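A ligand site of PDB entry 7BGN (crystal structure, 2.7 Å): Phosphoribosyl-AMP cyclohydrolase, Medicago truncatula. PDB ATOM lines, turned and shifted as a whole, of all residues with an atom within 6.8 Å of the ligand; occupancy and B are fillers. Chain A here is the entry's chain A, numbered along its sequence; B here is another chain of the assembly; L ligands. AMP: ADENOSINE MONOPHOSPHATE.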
ATOM      1  N   LEU A 131     -11.244   4.365   9.605  1.00  0.00           N
ATOM      2  CA  LEU A 131     -12.305   3.659  10.316  1.00  0.00           C
ATOM      3  C   LEU A 131     -13.491   4.575  10.618  1.00  0.00           C
ATOM      4  O   LEU A 131     -14.647   4.142  10.536  1.00  0.00           O
ATOM      5  CB  LEU A 131     -11.759   3.042  11.605  1.00  0.00           C
ATOM      6  CG  LEU A 131     -12.814   2.486  12.568  1.00  0.00           C
ATOM      7  CD1 LEU A 131     -13.615   1.362  11.929  1.00  0.00           C
ATOM      8  CD2 LEU A 131     -12.174   2.044  13.868  1.00  0.00           C
ATOM      9  N   THR A 134     -15.390   4.675   7.461  1.00  0.00           N
ATOM     10  CA  THR A 134     -16.178   3.465   7.242  1.00  0.00           C
ATOM     11  C   THR A 134     -17.461   3.500   8.066  1.00  0.00           C
ATOM     12  O   THR A 134     -18.558   3.273   7.536  1.00  0.00           O
ATOM     13  CB  THR A 134     -15.353   2.229   7.607  1.00  0.00           C
ATOM     14  OG1 THR A 134     -14.214   2.146   6.750  1.00  0.00           O
ATOM     15  CG2 THR A 134     -16.182   0.970   7.438  1.00  0.00           C
ATOM     16  N   ILE A 135     -17.339   3.821   9.352  1.00  0.00           N
ATOM     17  CA  ILE A 135     -18.505   3.928  10.218  1.00  0.00           C
ATOM     18  C   ILE A 135     -19.492   4.943   9.657  1.00  0.00           C
ATOM     19  O   ILE A 135     -20.711   4.718   9.693  1.00  0.00           O
ATOM     20  CB  ILE A 135     -18.049   4.296  11.640  1.00  0.00           C
ATOM     21  CG1 ILE A 135     -17.235   3.141  12.241  1.00  0.00           C
ATOM     22  CG2 ILE A 135     -19.240   4.689  12.510  1.00  0.00           C
ATOM     23  CD1 ILE A 135     -16.659   3.432  13.583  1.00  0.00           C
ATOM     24  N   ARG A 138     -21.571   3.302   6.868  1.00  0.00           N
ATOM     25  CA  ARG A 138     -22.629   2.439   7.373  1.00  0.00           C
ATOM     26  C   ARG A 138     -23.814   3.264   7.870  1.00  0.00           C
ATOM     27  O   ARG A 138     -24.974   2.867   7.678  1.00  0.00           O
ATOM     28  CB  ARG A 138     -22.094   1.566   8.504  1.00  0.00           C
ATOM     29  CG  ARG A 138     -20.930   0.728   8.093  1.00  0.00           C
ATOM     30  CD  ARG A 138     -21.319  -0.151   6.932  1.00  0.00           C
ATOM     31  NE  ARG A 138     -20.201  -0.291   6.003  1.00  0.00           N
ATOM     32  CZ  ARG A 138     -19.267  -1.221   6.111  1.00  0.00           C
ATOM     33  NH1 ARG A 138     -19.318  -2.082   7.117  1.00  0.00           N
ATOM     34  NH2 ARG A 138     -18.287  -1.284   5.234  1.00  0.00           N
ATOM     35  N   PRO A 149     -25.870  -7.246   5.788  1.00  0.00           N
ATOM     36  CA  PRO A 149     -25.721  -7.464   7.225  1.00  0.00           C
ATOM     37  C   PRO A 149     -24.435  -6.857   7.768  1.00  0.00           C
ATOM     38  O   PRO A 149     -23.355  -7.331   7.436  1.00  0.00           O
ATOM     39  CB  PRO A 149     -25.692  -8.989   7.342  1.00  0.00           C
ATOM     40  CG  PRO A 149     -25.181  -9.476   5.983  1.00  0.00           C
ATOM     41  CD  PRO A 149     -25.197  -8.308   5.017  1.00  0.00           C
ATOM     42  N   SER A 150     -24.530  -5.812   8.591  1.00  0.00           N
ATOM     43  CA  SER A 150     -23.332  -5.167   9.100  1.00  0.00           C
ATOM     44  C   SER A 150     -23.403  -4.977  10.602  1.00  0.00           C
ATOM     45  O   SER A 150     -24.469  -4.651  11.146  1.00  0.00           O
ATOM     46  CB  SER A 150     -23.126  -3.810   8.413  1.00  0.00           C
ATOM     47  OG  SER A 150     -22.490  -2.893   9.267  1.00  0.00           O
ATOM     48  N   TRP A 151     -22.261  -5.155  11.275  1.00  0.00           N
ATOM     49  CA  TRP A 151     -22.223  -4.972  12.718  1.00  0.00           C
ATOM     50  C   TRP A 151     -22.322  -3.512  13.090  1.00  0.00           C
ATOM     51  O   TRP A 151     -22.957  -3.172  14.096  1.00  0.00           O
ATOM     52  CB  TRP A 151     -20.962  -5.610  13.304  1.00  0.00           C
ATOM     53  CG  TRP A 151     -20.740  -5.373  14.767  1.00  0.00           C
ATOM     54  CD1 TRP A 151     -19.691  -4.699  15.338  1.00  0.00           C
ATOM     55  CD2 TRP A 151     -21.620  -5.722  15.852  1.00  0.00           C
ATOM     56  NE1 TRP A 151     -19.833  -4.664  16.705  1.00  0.00           N
ATOM     57  CE2 TRP A 151     -21.010  -5.281  17.044  1.00  0.00           C
ATOM     58  CE3 TRP A 151     -22.844  -6.389  15.926  1.00  0.00           C
ATOM     59  CZ2 TRP A 151     -21.593  -5.467  18.299  1.00  0.00           C
ATOM     60  CZ3 TRP A 151     -23.429  -6.579  17.172  1.00  0.00           C
ATOM     61  CH2 TRP A 151     -22.802  -6.123  18.344  1.00  0.00           C
ATOM     62  N   THR A 152     -21.754  -2.629  12.259  1.00  0.00           N
ATOM     63  CA  THR A 152     -21.892  -1.198  12.520  1.00  0.00           C
ATOM     64  C   THR A 152     -23.342  -0.761  12.349  1.00  0.00           C
ATOM     65  O   THR A 152     -23.854   0.006  13.172  1.00  0.00           O
ATOM     66  CB  THR A 152     -20.980  -0.410  11.600  1.00  0.00           C
ATOM     67  OG1 THR A 152     -19.646  -0.897  11.730  1.00  0.00           O
ATOM     68  CG2 THR A 152     -21.017   1.072  11.970  1.00  0.00           C
ATOM     69  N   LYS A 153     -24.003  -1.241  11.293  1.00  0.00           N
ATOM     70  CA  LYS A 153     -25.399  -0.901  11.110  1.00  0.00           C
ATOM     71  C   LYS A 153     -26.249  -1.448  12.235  1.00  0.00           C
ATOM     72  O   LYS A 153     -27.216  -0.803  12.651  1.00  0.00           O
ATOM     73  CB  LYS A 153     -25.913  -1.429   9.781  1.00  0.00           C
ATOM     74  CG  LYS A 153     -25.267  -0.782   8.598  1.00  0.00           C
ATOM     75  CD  LYS A 153     -26.003  -1.156   7.338  1.00  0.00           C
ATOM     76  CE  LYS A 153     -25.261  -0.675   6.123  1.00  0.00           C
ATOM     77  NZ  LYS A 153     -25.915  -1.135   4.883  1.00  0.00           N
ATOM     78  N   LEU A 155     -25.305  -1.686  15.350  1.00  0.00           N
ATOM     79  CA  LEU A 155     -25.105  -0.808  16.494  1.00  0.00           C
ATOM     80  C   LEU A 155     -25.782   0.551  16.288  1.00  0.00           C
ATOM     81  O   LEU A 155     -26.397   1.094  17.206  1.00  0.00           O
ATOM     82  CB  LEU A 155     -23.610  -0.609  16.756  1.00  0.00           C
ATOM     83  CG  LEU A 155     -22.847  -1.873  17.168  1.00  0.00           C
ATOM     84  CD1 LEU A 155     -21.340  -1.640  17.131  1.00  0.00           C
ATOM     85  CD2 LEU A 155     -23.304  -2.364  18.542  1.00  0.00           C
ATOM     86  N   LYS A 165     -22.534  -2.191  25.031  1.00  0.00           N
ATOM     87  CA  LYS A 165     -21.274  -2.676  24.470  1.00  0.00           C
ATOM     88  C   LYS A 165     -20.117  -1.780  24.879  1.00  0.00           C
ATOM     89  O   LYS A 165     -19.039  -2.263  25.228  1.00  0.00           O
ATOM     90  CB  LYS A 165     -21.386  -2.740  22.949  1.00  0.00           C
ATOM     91  CG  LYS A 165     -20.757  -3.932  22.235  1.00  0.00           C
ATOM     92  CD  LYS A 165     -19.861  -4.778  23.109  1.00  0.00           C
ATOM     93  CE  LYS A 165     -19.074  -5.802  22.284  1.00  0.00           C
ATOM     94  NZ  LYS A 165     -18.567  -6.876  23.176  1.00  0.00           N
ATOM     95  N   GLU A 169     -17.145  -3.113  27.166  1.00  0.00           N
ATOM     96  CA  GLU A 169     -15.774  -3.111  26.655  1.00  0.00           C
ATOM     97  C   GLU A 169     -14.869  -2.254  27.525  1.00  0.00           C
ATOM     98  O   GLU A 169     -13.687  -2.586  27.718  1.00  0.00           O
ATOM     99  CB  GLU A 169     -15.727  -2.628  25.205  1.00  0.00           C
ATOM    100  CG  GLU A 169     -16.305  -3.564  24.169  1.00  0.00           C
ATOM    101  CD  GLU A 169     -15.485  -4.828  23.965  1.00  0.00           C
ATOM    102  OE1 GLU A 169     -14.498  -5.026  24.685  1.00  0.00           O
ATOM    103  OE2 GLU A 169     -15.813  -5.604  23.036  1.00  0.00           O
ATOM    104  N   ALA A 191      -8.699  -1.100  21.460  1.00  0.00           N
ATOM    105  CA  ALA A 191      -9.306  -1.069  20.132  1.00  0.00           C
ATOM    106  C   ALA A 191     -10.799  -1.385  20.206  1.00  0.00           C
ATOM    107  O   ALA A 191     -11.603  -0.784  19.471  1.00  0.00           O
ATOM    108  CB  ALA A 191      -8.579  -2.052  19.220  1.00  0.00           C
ATOM    109  N   ASP A 192     -11.190  -2.339  21.061  1.00  0.00           N
ATOM    110  CA  ASP A 192     -12.599  -2.649  21.264  1.00  0.00           C
ATOM    111  C   ASP A 192     -13.361  -1.445  21.812  1.00  0.00           C
ATOM    112  O   ASP A 192     -14.519  -1.216  21.442  1.00  0.00           O
ATOM    113  CB  ASP A 192     -12.756  -3.832  22.204  1.00  0.00           C
ATOM    114  CG  ASP A 192     -12.293  -5.131  21.593  1.00  0.00           C
ATOM    115  OD1 ASP A 192     -11.807  -5.112  20.444  1.00  0.00           O
ATOM    116  OD2 ASP A 192     -12.433  -6.180  22.274  1.00  0.00           O
ATOM    117  N   TYR A 195     -13.533   1.406  18.838  1.00  0.00           N
ATOM    118  CA  TYR A 195     -14.462   1.184  17.727  1.00  0.00           C
ATOM    119  C   TYR A 195     -15.893   1.494  18.132  1.00  0.00           C
ATOM    120  O   TYR A 195     -16.610   2.214  17.431  1.00  0.00           O
ATOM    121  CB  TYR A 195     -14.325  -0.242  17.203  1.00  0.00           C
ATOM    122  CG  TYR A 195     -15.500  -0.636  16.348  1.00  0.00           C
ATOM    123  CD1 TYR A 195     -15.627  -0.131  15.067  1.00  0.00           C
ATOM    124  CD2 TYR A 195     -16.501  -1.474  16.828  1.00  0.00           C
ATOM    125  CE1 TYR A 195     -16.709  -0.465  14.287  1.00  0.00           C
ATOM    126  CE2 TYR A 195     -17.594  -1.810  16.042  1.00  0.00           C
ATOM    127  CZ  TYR A 195     -17.695  -1.296  14.783  1.00  0.00           C
ATOM    128  OH  TYR A 195     -18.763  -1.609  13.970  1.00  0.00           O
ATOM    129  N   HIS A 196     -16.354   0.916  19.254  1.00  0.00           N
ATOM    130  CA  HIS A 196     -17.737   1.093  19.671  1.00  0.00           C
ATOM    131  C   HIS A 196     -18.037   2.535  20.070  1.00  0.00           C
ATOM    132  O   HIS A 196     -19.121   3.047  19.777  1.00  0.00           O
ATOM    133  CB  HIS A 196     -18.047   0.138  20.822  1.00  0.00           C
ATOM    134  CG  HIS A 196     -17.962  -1.300  20.424  1.00  0.00           C
ATOM    135  ND1 HIS A 196     -16.808  -2.038  20.548  1.00  0.00           N
ATOM    136  CD2 HIS A 196     -18.877  -2.119  19.848  1.00  0.00           C
ATOM    137  CE1 HIS A 196     -17.016  -3.262  20.086  1.00  0.00           C
ATOM    138  NE2 HIS A 196     -18.259  -3.334  19.648  1.00  0.00           N
ATOM    139  N   VAL B 214      -3.960  -2.372  15.511  1.00  0.00           N
ATOM    140  CA  VAL B 214      -4.983  -3.398  15.725  1.00  0.00           C
ATOM    141  C   VAL B 214      -6.261  -3.044  14.960  1.00  0.00           C
ATOM    142  O   VAL B 214      -6.821  -3.874  14.231  1.00  0.00           O
ATOM    143  CB  VAL B 214      -5.250  -3.576  17.222  1.00  0.00           C
ATOM    144  CG1 VAL B 214      -6.463  -4.458  17.468  1.00  0.00           C
ATOM    145  CG2 VAL B 214      -4.019  -4.176  17.890  1.00  0.00           C
ATOM    146  N   LEU B 215      -6.696  -1.777  15.051  1.00  0.00           N
ATOM    147  CA  LEU B 215      -7.884  -1.351  14.303  1.00  0.00           C
ATOM    148  C   LEU B 215      -7.688  -1.584  12.816  1.00  0.00           C
ATOM    149  O   LEU B 215      -8.551  -2.189  12.152  1.00  0.00           O
ATOM    150  CB  LEU B 215      -8.161   0.122  14.575  1.00  0.00           C
ATOM    151  CG  LEU B 215      -8.776   0.395  15.938  1.00  0.00           C
ATOM    152  CD1 LEU B 215      -9.047   1.875  16.107  1.00  0.00           C
ATOM    153  CD2 LEU B 215     -10.059  -0.441  16.141  1.00  0.00           C
ATOM    154  N   ARG B 216      -6.536  -1.170  12.293  1.00  0.00           N
ATOM    155  CA  ARG B 216      -6.249  -1.337  10.869  1.00  0.00           C
ATOM    156  C   ARG B 216      -6.222  -2.809  10.498  1.00  0.00           C
ATOM    157  O   ARG B 216      -6.671  -3.199   9.409  1.00  0.00           O
ATOM    158  CB  ARG B 216      -4.936  -0.645  10.523  1.00  0.00           C
ATOM    159  CG  ARG B 216      -4.453  -0.903   9.123  1.00  0.00           C
ATOM    160  CD  ARG B 216      -3.251  -0.050   8.792  1.00  0.00           C
ATOM    161  NE  ARG B 216      -2.174  -0.216   9.750  1.00  0.00           N
ATOM    162  CZ  ARG B 216      -1.269  -1.193   9.664  1.00  0.00           C
ATOM    163  NH1 ARG B 216      -1.349  -2.068   8.673  1.00  0.00           N
ATOM    164  NH2 ARG B 216      -0.305  -1.298  10.564  1.00  0.00           N
ATOM    165  N   GLN B 217      -5.694  -3.653  11.380  1.00  0.00           N
ATOM    166  CA  GLN B 217      -5.700  -5.080  11.078  1.00  0.00           C
ATOM    167  C   GLN B 217      -7.095  -5.683  11.108  1.00  0.00           C
ATOM    168  O   GLN B 217      -7.288  -6.771  10.550  1.00  0.00           O
ATOM    169  CB  GLN B 217      -4.757  -5.813  12.032  1.00  0.00           C
ATOM    170  CG  GLN B 217      -3.264  -5.537  11.753  1.00  0.00           C
ATOM    171  CD  GLN B 217      -2.322  -6.058  12.828  1.00  0.00           C
ATOM    172  OE1 GLN B 217      -2.697  -6.266  13.971  1.00  0.00           O
ATOM    173  NE2 GLN B 217      -1.069  -6.282  12.439  1.00  0.00           N
ATOM    174  N   ARG B 218      -8.096  -5.008  11.676  1.00  0.00           N
ATOM    175  CA  ARG B 218      -9.452  -5.543  11.683  1.00  0.00           C
ATOM    176  C   ARG B 218     -10.296  -5.064  10.510  1.00  0.00           C
ATOM    177  O   ARG B 218     -11.498  -5.297  10.490  1.00  0.00           O
ATOM    178  CB  ARG B 218     -10.169  -5.178  12.985  1.00  0.00           C
ATOM    179  CG  ARG B 218      -9.554  -5.781  14.218  1.00  0.00           C
ATOM    180  CD  ARG B 218     -10.320  -5.378  15.477  1.00  0.00           C
ATOM    181  NE  ARG B 218      -9.599  -5.788  16.679  1.00  0.00           N
ATOM    182  CZ  ARG B 218      -9.952  -5.425  17.910  1.00  0.00           C
ATOM    183  NH1 ARG B 218     -11.019  -4.660  18.102  1.00  0.00           N
ATOM    184  NH2 ARG B 218      -9.220  -5.839  18.947  1.00  0.00           N
ATOM    185  N   PHE B 219      -9.681  -4.408   9.539  1.00  0.00           N
ATOM    186  CA  PHE B 219     -10.398  -3.983   8.352  1.00  0.00           C
ATOM    187  C   PHE B 219     -10.775  -5.210   7.530  1.00  0.00           C
ATOM    188  O   PHE B 219     -11.105  -5.098   6.353  1.00  0.00           O
ATOM    189  CB  PHE B 219      -9.554  -3.002   7.534  1.00  0.00           C
ATOM    190  CG  PHE B 219      -9.294  -1.674   8.230  1.00  0.00           C
ATOM    191  CD1 PHE B 219      -9.999  -1.312   9.367  1.00  0.00           C
ATOM    192  CD2 PHE B 219      -8.358  -0.783   7.726  1.00  0.00           C
ATOM    193  CE1 PHE B 219      -9.758  -0.097  10.011  1.00  0.00           C
ATOM    194  CE2 PHE B 219      -8.110   0.437   8.355  1.00  0.00           C
ATOM    195  CZ  PHE B 219      -8.815   0.780   9.498  1.00  0.00           C
HETATM  196  P   AMP L   1     -18.828  -3.896   9.510  1.00  0.00           P
HETATM  197  O1P AMP L   1     -18.829  -4.322   8.066  1.00  0.00           O
HETATM  198  O2P AMP L   1     -19.678  -2.683   9.815  1.00  0.00           O
HETATM  199  O3P AMP L   1     -19.148  -5.061  10.453  1.00  0.00           O
HETATM  200  O5' AMP L   1     -17.329  -3.484   9.869  1.00  0.00           O
HETATM  201  C5' AMP L   1     -16.651  -2.425   9.198  1.00  0.00           C
HETATM  202  C4' AMP L   1     -15.344  -2.095   9.888  1.00  0.00           C
HETATM  203  O4' AMP L   1     -15.612  -1.822  11.281  1.00  0.00           O
HETATM  204  C3' AMP L   1     -14.323  -3.214   9.931  1.00  0.00           C
HETATM  205  O3' AMP L   1     -13.568  -3.333   8.728  1.00  0.00           O
HETATM  206  C2' AMP L   1     -13.484  -2.881  11.157  1.00  0.00           C
HETATM  207  O2' AMP L   1     -12.493  -1.907  10.860  1.00  0.00           O
HETATM  208  C1' AMP L   1     -14.526  -2.235  12.073  1.00  0.00           C
HETATM  209  N9  AMP L   1     -15.038  -3.187  13.068  1.00  0.00           N
HETATM  210  C8  AMP L   1     -16.167  -3.958  12.957  1.00  0.00           C
HETATM  211  N7  AMP L   1     -16.398  -4.704  14.002  1.00  0.00           N
HETATM  212  C5  AMP L   1     -15.344  -4.421  14.851  1.00  0.00           C
HETATM  213  C6  AMP L   1     -15.008  -4.899  16.134  1.00  0.00           C
HETATM  214  N6  AMP L   1     -15.734  -5.806  16.786  1.00  0.00           N
HETATM  215  N1  AMP L   1     -13.886  -4.413  16.707  1.00  0.00           N
HETATM  216  C2  AMP L   1     -13.163  -3.499  16.043  1.00  0.00           C
HETATM  217  N3  AMP L   1     -13.385  -2.972  14.833  1.00  0.00           N
HETATM  218  C4  AMP L   1     -14.502  -3.480  14.288  1.00  0.00           C
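Residues that only touch the ligand: Leu 131 (3.6 Å), Thr 134 (3.9 Å), Tyr 195 (3.4 Å) and Phe 219 of chain B (3.0 Å).
Hydrophobic or aromatic side chains within 4 Å of the ligand: Leu 131, Trp 151, Tyr 195 and Phe 219 of chain B.
Nine residues have an atom within 4 Å of the ligand: Leu 131, Thr 134, Arg 138, Ser 150, Trp 151, Thr 152, Tyr 195, Arg 218 of chain B and Phe 219 of chain B.
The nearest printed residue that does not touch the ligand is Leu 215 of chain B (4.2 Å).
The side-chain hydroxyl of Ser 150 lies within hydrogen-bond range of the backbone NH of Thr 152 (3.1 Å).
The side-chain hydroxyl of Thr 152 is in hydrogen-bond range of the side-chain hydroxyl of Tyr 195.
N of Lys 153 lies within hydrogen-bond range of OG of Ser 150 (3.0 Å).
NH1 of Arg 218 of chain B is in salt-bridge range of OD1 of Asp 192 (2.5 Å).
An oxygen (O1P) of the ligand lies within salt-bridge range of the guanidinium group (NH1) of Arg 138, 2.5 Å away.
N of Thr 152 lies close to O2P of the ligand, 3.2 Å away.
OG1 of Thr 152 lies within hydrogen-bond range of O2P of the ligand, 2.6 Å away.
The side-chain hydroxyl (OG) of Ser 150 lies within hydrogen-bond range of an oxygen (O2P) of the ligand.
An oxygen (O3') of the ligand sits close to the backbone carbonyl oxygen of Arg 218 of chain B, 3.4 Å away.
The guanidinium group (NH1) of Arg 218 of chain B lies close to a nitrogen (N1) of the ligand (3.2 Å).
O3P of the ligand sits at hydrogen-bond distance from N of Trp 151, 3.2 Å away.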
